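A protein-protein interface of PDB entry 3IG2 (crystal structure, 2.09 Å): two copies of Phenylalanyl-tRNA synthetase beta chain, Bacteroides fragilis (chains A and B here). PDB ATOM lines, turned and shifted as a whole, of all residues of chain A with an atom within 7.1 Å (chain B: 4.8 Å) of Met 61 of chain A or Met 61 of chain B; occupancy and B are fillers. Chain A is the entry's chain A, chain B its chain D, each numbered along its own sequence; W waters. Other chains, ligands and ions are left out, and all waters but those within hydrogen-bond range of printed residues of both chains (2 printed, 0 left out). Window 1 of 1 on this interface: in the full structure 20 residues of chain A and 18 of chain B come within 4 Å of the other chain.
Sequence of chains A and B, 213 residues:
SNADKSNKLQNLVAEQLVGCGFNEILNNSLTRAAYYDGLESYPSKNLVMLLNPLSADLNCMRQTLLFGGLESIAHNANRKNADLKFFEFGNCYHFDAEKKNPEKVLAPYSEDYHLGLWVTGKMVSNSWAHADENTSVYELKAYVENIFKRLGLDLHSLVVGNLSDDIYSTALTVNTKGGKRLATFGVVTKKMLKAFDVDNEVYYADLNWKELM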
ATOM      1  N   ASN A  28     -18.339  10.468 -10.981  1.00  0.00           N
ATOM      2  CA  ASN A  28     -19.801  10.590 -10.846  1.00  0.00           C
ATOM      3  C   ASN A  28     -20.519   9.473 -11.564  1.00  0.00           C
ATOM      4  O   ASN A  28     -20.163   9.109 -12.689  1.00  0.00           O
ATOM      5  CB  ASN A  28     -20.255  11.922 -11.466  1.00  0.00           C
ATOM      6  CG  ASN A  28     -21.601  12.443 -10.900  1.00  0.00           C
ATOM      7  OD1 ASN A  28     -21.868  13.643 -11.004  1.00  0.00           O
ATOM      8  ND2 ASN A  28     -22.444  11.555 -10.310  1.00  0.00           N
ATOM      9  N   SER A  29     -21.544   8.922 -10.924  1.00  0.00           N
ATOM     10  CA  SER A  29     -22.308   7.881 -11.590  1.00  0.00           C
ATOM     11  C   SER A  29     -23.216   8.485 -12.674  1.00  0.00           C
ATOM     12  O   SER A  29     -23.554   7.799 -13.630  1.00  0.00           O
ATOM     13  CB  SER A  29     -23.046   7.025 -10.585  1.00  0.00           C
ATOM     14  OG  SER A  29     -22.091   6.322  -9.783  1.00  0.00           O
ATOM     15  N   LEU A  30     -23.551   9.768 -12.537  1.00  0.00           N
ATOM     16  CA  LEU A  30     -24.211  10.518 -13.613  1.00  0.00           C
ATOM     17  C   LEU A  30     -23.225  10.840 -14.751  1.00  0.00           C
ATOM     18  O   LEU A  30     -22.072  11.269 -14.508  1.00  0.00           O
ATOM     19  CB  LEU A  30     -24.830  11.820 -13.083  1.00  0.00           C
ATOM     20  CG  LEU A  30     -25.922  11.743 -12.004  1.00  0.00           C
ATOM     21  CD1 LEU A  30     -25.906  12.994 -11.186  1.00  0.00           C
ATOM     22  CD2 LEU A  30     -27.261  11.606 -12.664  1.00  0.00           C
ATOM     23  N   THR A  31     -23.689  10.658 -15.988  1.00  0.00           N
ATOM     24  CA  THR A  31     -22.816  10.757 -17.141  1.00  0.00           C
ATOM     25  C   THR A  31     -23.578  11.205 -18.397  1.00  0.00           C
ATOM     26  O   THR A  31     -24.705  11.669 -18.291  1.00  0.00           O
ATOM     27  CB  THR A  31     -22.093   9.410 -17.367  1.00  0.00           C
ATOM     28  OG1 THR A  31     -21.074   9.573 -18.355  1.00  0.00           O
ATOM     29  CG2 THR A  31     -23.073   8.332 -17.795  1.00  0.00           C
ATOM     30  N   ARG A  32     -22.959  11.095 -19.568  1.00  0.00           N
ATOM     31  CA  ARG A  32     -23.528  11.661 -20.783  1.00  0.00           C
ATOM     32  C   ARG A  32     -23.904  10.555 -21.751  1.00  0.00           C
ATOM     33  O   ARG A  32     -23.059   9.721 -22.109  1.00  0.00           O
ATOM     34  CB  ARG A  32     -22.546  12.608 -21.472  1.00  0.00           C
ATOM     35  CG  ARG A  32     -22.093  13.770 -20.639  1.00  0.00           C
ATOM     36  CD  ARG A  32     -20.924  14.455 -21.329  1.00  0.00           C
ATOM     37  NE  ARG A  32     -20.774  15.832 -20.900  1.00  0.00           N
ATOM     38  CZ  ARG A  32     -21.347  16.870 -21.506  1.00  0.00           C
ATOM     39  NH1 ARG A  32     -22.112  16.682 -22.573  1.00  0.00           N
ATOM     40  NH2 ARG A  32     -21.150  18.103 -21.053  1.00  0.00           N
ATOM     41  N   TYR A  36     -22.203   7.013 -25.378  1.00  0.00           N
ATOM     42  CA  TYR A  36     -22.567   5.691 -25.789  1.00  0.00           C
ATOM     43  C   TYR A  36     -23.031   5.653 -27.240  1.00  0.00           C
ATOM     44  O   TYR A  36     -23.305   4.569 -27.758  1.00  0.00           O
ATOM     45  CB  TYR A  36     -23.614   5.137 -24.826  1.00  0.00           C
ATOM     46  CG  TYR A  36     -23.092   5.008 -23.396  1.00  0.00           C
ATOM     47  CD1 TYR A  36     -22.700   3.780 -22.896  1.00  0.00           C
ATOM     48  CD2 TYR A  36     -22.999   6.123 -22.544  1.00  0.00           C
ATOM     49  CE1 TYR A  36     -22.203   3.648 -21.570  1.00  0.00           C
ATOM     50  CE2 TYR A  36     -22.513   6.003 -21.224  1.00  0.00           C
ATOM     51  CZ  TYR A  36     -22.104   4.762 -20.751  1.00  0.00           C
ATOM     52  OH  TYR A  36     -21.631   4.614 -19.448  1.00  0.00           O
ATOM     53  N   ASN A  46     -29.529   0.545 -23.719  1.00  0.00           N
ATOM     54  CA  ASN A  46     -29.474  -0.085 -22.389  1.00  0.00           C
ATOM     55  C   ASN A  46     -29.134   0.927 -21.309  1.00  0.00           C
ATOM     56  O   ASN A  46     -28.971   0.582 -20.147  1.00  0.00           O
ATOM     57  CB  ASN A  46     -28.510  -1.280 -22.363  1.00  0.00           C
ATOM     58  CG  ASN A  46     -28.984  -2.439 -23.225  1.00  0.00           C
ATOM     59  OD1 ASN A  46     -28.199  -3.042 -23.951  1.00  0.00           O
ATOM     60  ND2 ASN A  46     -30.259  -2.774 -23.132  1.00  0.00           N
ATOM     61  N   LEU A  47     -29.025   2.191 -21.704  1.00  0.00           N
ATOM     62  CA  LEU A  47     -28.727   3.255 -20.758  1.00  0.00           C
ATOM     63  C   LEU A  47     -29.937   3.480 -19.883  1.00  0.00           C
ATOM     64  O   LEU A  47     -31.075   3.425 -20.360  1.00  0.00           O
ATOM     65  CB  LEU A  47     -28.426   4.559 -21.492  1.00  0.00           C
ATOM     66  CG  LEU A  47     -27.069   4.750 -22.147  1.00  0.00           C
ATOM     67  CD1 LEU A  47     -27.116   6.066 -22.896  1.00  0.00           C
ATOM     68  CD2 LEU A  47     -25.994   4.752 -21.084  1.00  0.00           C
ATOM     69  N   VAL A  48     -29.680   3.719 -18.598  1.00  0.00           N
ATOM     70  CA  VAL A  48     -30.707   4.175 -17.672  1.00  0.00           C
ATOM     71  C   VAL A  48     -30.791   5.693 -17.775  1.00  0.00           C
ATOM     72  O   VAL A  48     -29.992   6.432 -17.153  1.00  0.00           O
ATOM     73  CB  VAL A  48     -30.318   3.790 -16.250  1.00  0.00           C
ATOM     74  CG1 VAL A  48     -31.314   4.391 -15.258  1.00  0.00           C
ATOM     75  CG2 VAL A  48     -30.248   2.260 -16.105  1.00  0.00           C
ATOM     76  N   MET A  49     -31.703   6.177 -18.592  1.00  0.00           N
ATOM     77  CA  MET A  49     -31.817   7.610 -18.813  1.00  0.00           C
ATOM     78  C   MET A  49     -32.536   8.309 -17.651  1.00  0.00           C
ATOM     79  O   MET A  49     -33.319   7.706 -16.958  1.00  0.00           O
ATOM     80  CB  MET A  49     -32.577   7.878 -20.111  1.00  0.00           C
ATOM     81  CG  MET A  49     -32.026   7.154 -21.321  1.00  0.00           C
ATOM     82  SD  MET A  49     -30.390   7.972 -21.908  1.00  0.00           S
ATOM     83  CE  MET A  49     -30.986   9.830 -21.890  1.00  0.00           C
ATOM     84  N   LEU A  50     -32.250   9.586 -17.460  1.00  0.00           N
ATOM     85  CA  LEU A  50     -32.969  10.425 -16.495  1.00  0.00           C
ATOM     86  C   LEU A  50     -34.225  11.015 -17.131  1.00  0.00           C
ATOM     87  O   LEU A  50     -34.284  11.242 -18.333  1.00  0.00           O
ATOM     88  CB  LEU A  50     -32.087  11.604 -16.064  1.00  0.00           C
ATOM     89  CG  LEU A  50     -31.075  11.518 -14.916  1.00  0.00           C
ATOM     90  CD1 LEU A  50     -30.731  10.116 -14.432  1.00  0.00           C
ATOM     91  CD2 LEU A  50     -29.837  12.345 -15.165  1.00  0.00           C
ATOM     92  N   ASN A  59     -27.331  13.332 -18.218  1.00  0.00           N
ATOM     93  CA  ASN A  59     -28.660  12.900 -18.626  1.00  0.00           C
ATOM     94  C   ASN A  59     -28.948  11.395 -18.471  1.00  0.00           C
ATOM     95  O   ASN A  59     -30.008  10.928 -18.868  1.00  0.00           O
ATOM     96  CB  ASN A  59     -28.952  13.388 -20.056  1.00  0.00           C
ATOM     97  CG  ASN A  59     -27.868  13.007 -21.041  1.00  0.00           C
ATOM     98  OD1 ASN A  59     -27.135  12.030 -20.839  1.00  0.00           O
ATOM     99  ND2 ASN A  59     -27.762  13.773 -22.134  1.00  0.00           N
ATOM    100  N   CYS A  60     -27.990  10.644 -17.908  1.00  0.00           N
ATOM    101  CA  CYS A  60     -28.162   9.199 -17.690  1.00  0.00           C
ATOM    102  C   CYS A  60     -27.213   8.705 -16.607  1.00  0.00           C
ATOM    103  O   CYS A  60     -26.321   9.445 -16.184  1.00  0.00           O
ATOM    104  CB  CYS A  60     -27.893   8.409 -18.979  1.00  0.00           C
ATOM    105  SG  CYS A  60     -26.244   8.573 -19.579  1.00  0.00           S
ATOM    106  N   MET A  61     -27.422   7.464 -16.171  1.00  0.00           N
ATOM    107  CA  MET A  61     -26.499   6.788 -15.261  1.00  0.00           C
ATOM    108  C   MET A  61     -25.470   5.978 -16.075  1.00  0.00           C
ATOM    109  O   MET A  61     -25.792   5.459 -17.141  1.00  0.00           O
ATOM    110  CB  MET A  61     -27.274   5.878 -14.316  1.00  0.00           C
ATOM    111  CG  MET A  61     -28.420   6.570 -13.621  1.00  0.00           C
ATOM    112  SD  MET A  61     -27.893   8.101 -12.519  1.00  0.00           S
ATOM    113  CE  MET A  61     -26.633   7.242 -11.310  1.00  0.00           C
ATOM    114  N   ARG A  62     -24.234   5.885 -15.587  1.00  0.00           N
ATOM    115  CA  ARG A  62     -23.209   5.136 -16.323  1.00  0.00           C
ATOM    116  C   ARG A  62     -23.522   3.629 -16.408  1.00  0.00           C
ATOM    117  O   ARG A  62     -24.041   3.037 -15.469  1.00  0.00           O
ATOM    118  CB  ARG A  62     -21.822   5.393 -15.732  1.00  0.00           C
ATOM    119  CG  ARG A  62     -21.708   4.946 -14.255  1.00  0.00           C
ATOM    120  CD  ARG A  62     -20.322   5.196 -13.666  1.00  0.00           C
ATOM    121  NE  ARG A  62     -20.286   4.707 -12.291  1.00  0.00           N
ATOM    122  CZ  ARG A  62     -19.391   5.087 -11.383  1.00  0.00           C
ATOM    123  NH1 ARG A  62     -18.452   5.970 -11.689  1.00  0.00           N
ATOM    124  NH2 ARG A  62     -19.459   4.605 -10.149  1.00  0.00           N
ATOM    125  N   GLN A  63     -23.259   3.057 -17.590  1.00  0.00           N
ATOM    126  CA  GLN A  63     -23.265   1.633 -17.870  1.00  0.00           C
ATOM    127  C   GLN A  63     -21.891   1.010 -17.670  1.00  0.00           C
ATOM    128  O   GLN A  63     -21.790  -0.188 -17.473  1.00  0.00           O
ATOM    129  CB  GLN A  63     -23.635   1.410 -19.342  1.00  0.00           C
ATOM    130  CG  GLN A  63     -24.960   0.780 -19.584  1.00  0.00           C
ATOM    131  CD  GLN A  63     -25.196   0.392 -21.041  1.00  0.00           C
ATOM    132  OE1 GLN A  63     -25.111  -0.781 -21.394  1.00  0.00           O
ATOM    133  NE2 GLN A  63     -25.508   1.372 -21.884  1.00  0.00           N
ATOM    134  N   THR A  64     -20.841   1.814 -17.794  1.00  0.00           N
ATOM    135  CA  THR A  64     -19.447   1.358 -17.715  1.00  0.00           C
ATOM    136  C   THR A  64     -18.643   2.397 -16.936  1.00  0.00           C
ATOM    137  O   THR A  64     -18.946   3.592 -17.016  1.00  0.00           O
ATOM    138  CB  THR A  64     -18.804   1.191 -19.119  1.00  0.00           C
ATOM    139  OG1 THR A  64     -17.431   0.805 -18.958  1.00  0.00           O
ATOM    140  CG2 THR A  64     -18.879   2.494 -19.960  1.00  0.00           C
ATOM    141  N   ASN A  91     -20.644   1.528  -8.694  1.00  0.00           N
ATOM    142  CA  ASN A  91     -21.809   0.965  -9.319  1.00  0.00           C
ATOM    143  C   ASN A  91     -21.960   1.425 -10.764  1.00  0.00           C
ATOM    144  O   ASN A  91     -21.677   2.602 -11.085  1.00  0.00           O
ATOM    145  CB  ASN A  91     -23.059   1.354  -8.528  1.00  0.00           C
ATOM    146  CG  ASN A  91     -23.159   0.609  -7.217  1.00  0.00           C
ATOM    147  OD1 ASN A  91     -23.285   1.221  -6.156  1.00  0.00           O
ATOM    148  ND2 ASN A  91     -23.076  -0.726  -7.280  1.00  0.00           N
ATOM    149  N   CYS A  92     -22.388   0.488 -11.616  1.00  0.00           N
ATOM    150  CA  CYS A  92     -22.895   0.792 -12.953  1.00  0.00           C
ATOM    151  C   CYS A  92     -24.359   0.368 -13.067  1.00  0.00           C
ATOM    152  O   CYS A  92     -24.849  -0.449 -12.281  1.00  0.00           O
ATOM    153  CB  CYS A  92     -22.059   0.092 -14.024  1.00  0.00           C
ATOM    154  SG  CYS A  92     -20.336   0.733 -14.136  1.00  0.00           S
ATOM    155  N   TYR A  93     -25.046   0.899 -14.076  1.00  0.00           N
ATOM    156  CA  TYR A  93     -26.492   0.802 -14.165  1.00  0.00           C
ATOM    157  C   TYR A  93     -26.883   0.358 -15.557  1.00  0.00           C
ATOM    158  O   TYR A  93     -26.293   0.784 -16.554  1.00  0.00           O
ATOM    159  CB  TYR A  93     -27.135   2.140 -13.778  1.00  0.00           C
ATOM    160  CG  TYR A  93     -26.733   2.539 -12.382  1.00  0.00           C
ATOM    161  CD1 TYR A  93     -27.532   2.216 -11.298  1.00  0.00           C
ATOM    162  CD2 TYR A  93     -25.522   3.193 -12.148  1.00  0.00           C
ATOM    163  CE1 TYR A  93     -27.144   2.543 -10.018  1.00  0.00           C
ATOM    164  CE2 TYR A  93     -25.115   3.508 -10.873  1.00  0.00           C
ATOM    165  CZ  TYR A  93     -25.941   3.195  -9.807  1.00  0.00           C
ATOM    166  OH  TYR A  93     -25.561   3.498  -8.528  1.00  0.00           O
ATOM    167  N   HIS A  94     -27.879  -0.510 -15.618  1.00  0.00           N
ATOM    168  CA  HIS A  94     -28.271  -1.204 -16.861  1.00  0.00           C
ATOM    169  C   HIS A  94     -29.784  -1.132 -16.978  1.00  0.00           C
ATOM    170  O   HIS A  94     -30.488  -1.398 -15.996  1.00  0.00           O
ATOM    171  CB  HIS A  94     -27.854  -2.704 -16.851  1.00  0.00           C
ATOM    172  CG  HIS A  94     -28.193  -3.442 -18.114  1.00  0.00           C
ATOM    173  ND1 HIS A  94     -27.429  -3.351 -19.258  1.00  0.00           N
ATOM    174  CD2 HIS A  94     -29.221  -4.275 -18.414  1.00  0.00           C
ATOM    175  CE1 HIS A  94     -27.967  -4.100 -20.205  1.00  0.00           C
ATOM    176  NE2 HIS A  94     -29.057  -4.665 -19.720  1.00  0.00           N
ATOM    177  N   GLU A 111     -28.477  -2.453 -10.862  1.00  0.00           N
ATOM    178  CA  GLU A 111     -27.142  -1.956 -10.559  1.00  0.00           C
ATOM    179  C   GLU A 111     -26.193  -3.096 -10.235  1.00  0.00           C
ATOM    180  O   GLU A 111     -26.602  -4.094  -9.666  1.00  0.00           O
ATOM    181  CB  GLU A 111     -27.132  -0.878  -9.455  1.00  0.00           C
ATOM    182  CG  GLU A 111     -27.563  -1.281  -8.079  1.00  0.00           C
ATOM    183  CD  GLU A 111     -27.802  -0.050  -7.193  1.00  0.00           C
ATOM    184  OE1 GLU A 111     -26.819   0.464  -6.589  1.00  0.00           O
ATOM    185  OE2 GLU A 111     -28.983   0.393  -7.103  1.00  0.00           O
ATOM    186  N   SER B  29     -28.427   1.999  -4.734  1.00  0.00           N
ATOM    187  CA  SER B  29     -28.691   3.403  -5.003  1.00  0.00           C
ATOM    188  C   SER B  29     -30.026   3.602  -5.714  1.00  0.00           C
ATOM    189  O   SER B  29     -30.621   4.663  -5.594  1.00  0.00           O
ATOM    190  CB  SER B  29     -27.564   4.016  -5.808  1.00  0.00           C
ATOM    191  OG  SER B  29     -26.402   4.074  -5.025  1.00  0.00           O
ATOM    192  N   LEU B  30     -30.472   2.587  -6.454  1.00  0.00           N
ATOM    193  CA  LEU B  30     -31.788   2.593  -7.072  1.00  0.00           C
ATOM    194  C   LEU B  30     -32.859   2.434  -5.993  1.00  0.00           C
ATOM    195  O   LEU B  30     -32.731   1.591  -5.104  1.00  0.00           O
ATOM    196  CB  LEU B  30     -31.924   1.473  -8.111  1.00  0.00           C
ATOM    197  CG  LEU B  30     -31.158   1.619  -9.425  1.00  0.00           C
ATOM    198  CD1 LEU B  30     -31.226   0.332 -10.201  1.00  0.00           C
ATOM    199  CD2 LEU B  30     -31.654   2.772 -10.263  1.00  0.00           C
ATOM    200  N   THR B  31     -33.890   3.268  -6.060  1.00  0.00           N
ATOM    201  CA  THR B  31     -34.871   3.329  -4.986  1.00  0.00           C
ATOM    202  C   THR B  31     -36.295   3.648  -5.476  1.00  0.00           C
ATOM    203  O   THR B  31     -36.524   3.780  -6.682  1.00  0.00           O
ATOM    204  CB  THR B  31     -34.401   4.299  -3.879  1.00  0.00           C
ATOM    205  OG1 THR B  31     -35.086   3.982  -2.662  1.00  0.00           O
ATOM    206  CG2 THR B  31     -34.644   5.782  -4.271  1.00  0.00           C
ATOM    207  N   LEU B  47     -35.984  14.871  -6.285  1.00  0.00           N
ATOM    208  CA  LEU B  47     -35.574  13.517  -6.663  1.00  0.00           C
ATOM    209  C   LEU B  47     -34.994  13.477  -8.066  1.00  0.00           C
ATOM    210  O   LEU B  47     -35.520  14.110  -8.997  1.00  0.00           O
ATOM    211  CB  LEU B  47     -36.751  12.527  -6.618  1.00  0.00           C
ATOM    212  CG  LEU B  47     -37.166  11.884  -5.307  1.00  0.00           C
ATOM    213  CD1 LEU B  47     -38.375  10.973  -5.504  1.00  0.00           C
ATOM    214  CD2 LEU B  47     -36.033  11.120  -4.648  1.00  0.00           C
ATOM    215  N   VAL B  48     -33.918  12.704  -8.212  1.00  0.00           N
ATOM    216  CA  VAL B  48     -33.362  12.386  -9.524  1.00  0.00           C
ATOM    217  C   VAL B  48     -34.150  11.204 -10.045  1.00  0.00           C
ATOM    218  O   VAL B  48     -33.920  10.059  -9.661  1.00  0.00           O
ATOM    219  CB  VAL B  48     -31.867  12.079  -9.445  1.00  0.00           C
ATOM    220  CG1 VAL B  48     -31.316  11.666 -10.816  1.00  0.00           C
ATOM    221  CG2 VAL B  48     -31.105  13.298  -8.907  1.00  0.00           C
ATOM    222  N   LEU B  50     -35.957   8.706 -12.926  1.00  0.00           N
ATOM    223  CA  LEU B  50     -35.521   7.974 -14.093  1.00  0.00           C
ATOM    224  C   LEU B  50     -36.617   8.005 -15.155  1.00  0.00           C
ATOM    225  O   LEU B  50     -37.757   8.346 -14.856  1.00  0.00           O
ATOM    226  CB  LEU B  50     -35.192   6.542 -13.690  1.00  0.00           C
ATOM    227  CG  LEU B  50     -33.790   6.217 -13.157  1.00  0.00           C
ATOM    228  CD1 LEU B  50     -32.927   7.413 -12.749  1.00  0.00           C
ATOM    229  CD2 LEU B  50     -33.788   5.150 -12.103  1.00  0.00           C
ATOM    230  N   ASN B  59     -37.446   3.508  -9.495  1.00  0.00           N
ATOM    231  CA  ASN B  59     -37.652   4.487 -10.541  1.00  0.00           C
ATOM    232  C   ASN B  59     -36.956   5.828 -10.321  1.00  0.00           C
ATOM    233  O   ASN B  59     -37.257   6.814 -11.010  1.00  0.00           O
ATOM    234  CB  ASN B  59     -39.153   4.692 -10.747  1.00  0.00           C
ATOM    235  CG  ASN B  59     -39.837   5.205  -9.506  1.00  0.00           C
ATOM    236  OD1 ASN B  59     -39.200   5.443  -8.456  1.00  0.00           O
ATOM    237  ND2 ASN B  59     -41.145   5.376  -9.600  1.00  0.00           N
ATOM    238  N   CYS B  60     -36.052   5.871  -9.344  1.00  0.00           N
ATOM    239  CA  CYS B  60     -35.329   7.083  -9.011  1.00  0.00           C
ATOM    240  C   CYS B  60     -34.058   6.712  -8.260  1.00  0.00           C
ATOM    241  O   CYS B  60     -33.862   5.546  -7.843  1.00  0.00           O
ATOM    242  CB  CYS B  60     -36.191   8.035  -8.170  1.00  0.00           C
ATOM    243  SG  CYS B  60     -36.495   7.484  -6.470  1.00  0.00           S
ATOM    244  N   MET B  61     -33.194   7.707  -8.092  1.00  0.00           N
ATOM    245  CA  MET B  61     -31.984   7.542  -7.315  1.00  0.00           C
ATOM    246  C   MET B  61     -32.249   8.041  -5.907  1.00  0.00           C
ATOM    247  O   MET B  61     -33.037   8.975  -5.714  1.00  0.00           O
ATOM    248  CB  MET B  61     -30.830   8.311  -7.941  1.00  0.00           C
ATOM    249  CG  MET B  61     -30.537   7.919  -9.380  1.00  0.00           C
ATOM    250  SD  MET B  61     -29.995   6.091  -9.646  1.00  0.00           S
ATOM    251  CE  MET B  61     -28.475   5.972  -8.548  1.00  0.00           C
ATOM    252  N   ARG B  62     -31.579   7.432  -4.931  1.00  0.00           N
ATOM    253  CA  ARG B  62     -31.830   7.765  -3.535  1.00  0.00           C
ATOM    254  C   ARG B  62     -31.362   9.174  -3.237  1.00  0.00           C
ATOM    255  O   ARG B  62     -30.309   9.597  -3.720  1.00  0.00           O
ATOM    256  CB  ARG B  62     -31.181   6.750  -2.577  1.00  0.00           C
ATOM    257  CG  ARG B  62     -29.657   6.727  -2.617  1.00  0.00           C
ATOM    258  CD  ARG B  62     -29.073   5.673  -1.712  1.00  0.00           C
ATOM    259  NE  ARG B  62     -27.618   5.632  -1.878  1.00  0.00           N
ATOM    260  CZ  ARG B  62     -26.846   4.631  -1.480  1.00  0.00           C
ATOM    261  NH1 ARG B  62     -27.380   3.572  -0.907  1.00  0.00           N
ATOM    262  NH2 ARG B  62     -25.533   4.689  -1.666  1.00  0.00           N
ATOM    263  N   GLN B  63     -32.178   9.892  -2.464  1.00  0.00           N
ATOM    264  CA  GLN B  63     -31.873  11.236  -1.991  1.00  0.00           C
ATOM    265  C   GLN B  63     -31.302  11.167  -0.562  1.00  0.00           C
ATOM    266  O   GLN B  63     -30.589  12.063  -0.142  1.00  0.00           O
ATOM    267  CB  GLN B  63     -33.142  12.069  -1.987  1.00  0.00           C
ATOM    268  CG  GLN B  63     -32.877  13.542  -2.177  1.00  0.00           C
ATOM    269  CD  GLN B  63     -34.119  14.386  -2.145  1.00  0.00           C
ATOM    270  OE1 GLN B  63     -35.176  13.995  -2.654  1.00  0.00           O
ATOM    271  NE2 GLN B  63     -34.012  15.551  -1.533  1.00  0.00           N
ATOM    272  N   TYR B  93     -28.241  11.359  -4.324  1.00  0.00           N
ATOM    273  CA  TYR B  93     -28.452  12.163  -5.526  1.00  0.00           C
ATOM    274  C   TYR B  93     -29.553  13.208  -5.320  1.00  0.00           C
ATOM    275  O   TYR B  93     -30.529  12.968  -4.607  1.00  0.00           O
ATOM    276  CB  TYR B  93     -28.702  11.248  -6.739  1.00  0.00           C
ATOM    277  CG  TYR B  93     -27.545  10.290  -6.949  1.00  0.00           C
ATOM    278  CD1 TYR B  93     -26.514  10.606  -7.817  1.00  0.00           C
ATOM    279  CD2 TYR B  93     -27.455   9.091  -6.226  1.00  0.00           C
ATOM    280  CE1 TYR B  93     -25.437   9.749  -7.992  1.00  0.00           C
ATOM    281  CE2 TYR B  93     -26.374   8.247  -6.380  1.00  0.00           C
ATOM    282  CZ  TYR B  93     -25.368   8.586  -7.262  1.00  0.00           C
ATOM    283  OH  TYR B  93     -24.288   7.760  -7.441  1.00  0.00           O
HETATM  284  O   HOH W   1     -25.474   1.565  -4.002  1.00  0.00           O
HETATM  285  O   HOH W   2     -23.561   4.892  -8.011  1.00  0.00           O
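The side-chain carboxylate (OE1) of Glu 111 of chain A lies within hydrogen-bond range of the backbone NH (N) of Ser 29 of chain B (2.9 Å).
The side-chain carboxylate (OE2) of Glu 111 of chain A is in hydrogen-bond range of the backbone NH (N) of Leu 30 of chain B (2.7 Å).
The backbone NH (N) of Met 61 of chain A lies within hydrogen-bond range of the backbone carbonyl oxygen (O) of Val 48 of chain A.
The backbone carbonyl oxygen of Asn 59 of chain A is in hydrogen-bond range of the backbone NH of Leu 50 of chain A, at 3.0 Å.
The backbone carbonyl oxygen (O) of Ser 29 of chain B is in hydrogen-bond range of the backbone NH (N) of Arg 62 of chain B, at 3.0 Å.
The backbone carbonyl oxygen of Val 48 of chain B sits at hydrogen-bond distance from the backbone NH of Met 61 of chain B (2.9 Å).
The backbone NH (N) of Leu 50 of chain B sits at hydrogen-bond distance from the backbone carbonyl oxygen (O) of Asn 59 of chain B.
N of Tyr 93 of chain B is in hydrogen-bond range of O of Arg 62 of chain B.
Among the printed residues, merely in contact across the chains: Tyr 93 of chain A with Ser 29 of chain B, Ser 29 of chain A with Tyr 93 of chain B, Met 61 of chain A with Met 61 of chain B, Met 49 of chain A with Leu 50 of chain B, Val 48 of chain A with Leu 50 of chain B, Tyr 93 of chain A with Met 61 of chain B, Leu 50 of chain A with Leu 50 of chain B and Leu 50 of chain A with Val 48 of chain B.
Printed residues of chain B within 4 Å of Met 61 of chain A: Met 61 (3.6 Å).
Of chain A, only Met 61 (3.6 Å) and Tyr 93 (3.8 Å) come within 4 Å of Met 61 of chain B.
Printed residues of chain A within 4 Å of Leu 30 of chain B: Glu 111.
Of the printed residues of chain B, Met 49 of chain A touches Leu 50.
Of the printed residues of chain B, Tyr 93 of chain A touches Ser 29 (3.4 Å) and Met 61 (3.8 Å).
Printed residues of chain B within 4 Å of Val 48 of chain A: Leu 50.
Of the printed residues of chain A, Val 48 of chain B touches Leu 50 (3.98 Å).
Arg 62 of chain A touches none of the printed residues of chain B.
Leu 47 of chain A touches none of the printed residues of chain B.
The nearest residue of chain B that does not touch Met 61 of chain A is Tyr 93 of chain B (4.3 Å).
The nearest residue of chain A that does not touch Met 61 of chain B is Leu 50 of chain A (5.5 Å).
Of the 22 printed residues of chain A, 7 touch a printed residue of chain B.
Printed residues of chain A that touch a printed residue of chain B: Ser 29, Val 48, Met 49, Leu 50, Met 61, Tyr 93 and Glu 111.
Hydrophobic or aromatic side chains of chain A within 4 Å of the printed part of chain B: Val 48, Leu 50, Met 61 and Tyr 93.
Among the printed residues, no Asp or Glu carboxylate lies within 4 Å of a Lys or Arg side-chain nitrogen of the other chain.
Ser 29 of chain A touches Tyr 93 of chain B, and with the chains exchanged Tyr 93 of chain A touches Ser 29 of chain B.
Val 48 of chain A touches Leu 50 of chain B, and with the chains exchanged Leu 50 of chain A touches Val 48 of chain B.
Leu 50 of chain A touches its own counterpart, Leu 50 of chain B.
Tyr 93 of chain A touches Met 61 of chain B, but with the chains exchanged Met 61 of chain A does not touch Tyr 93 of chain B (4.3 Å).
12 positions are printed for both chains.
Of the 10 pairs that touch across the chains among the printed residues, 6 have their exchanged pair printed and touching as well.
Water W2 lies within hydrogen-bond range of the side-chain hydroxyl of Tyr 93 of chain A (2.5 Å), the side-chain hydroxyl of Ser 29 of chain A (2.7 Å) and the side-chain hydroxyl of Tyr 93 of chain B (3.0 Å).
Water W1 lies within hydrogen-bond range of OG of Ser 29 of chain B (2.9 Å), OD1 of Asn 91 of chain A (3.1 Å) and OE1 of Glu 111 of chain A (3.1 Å).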
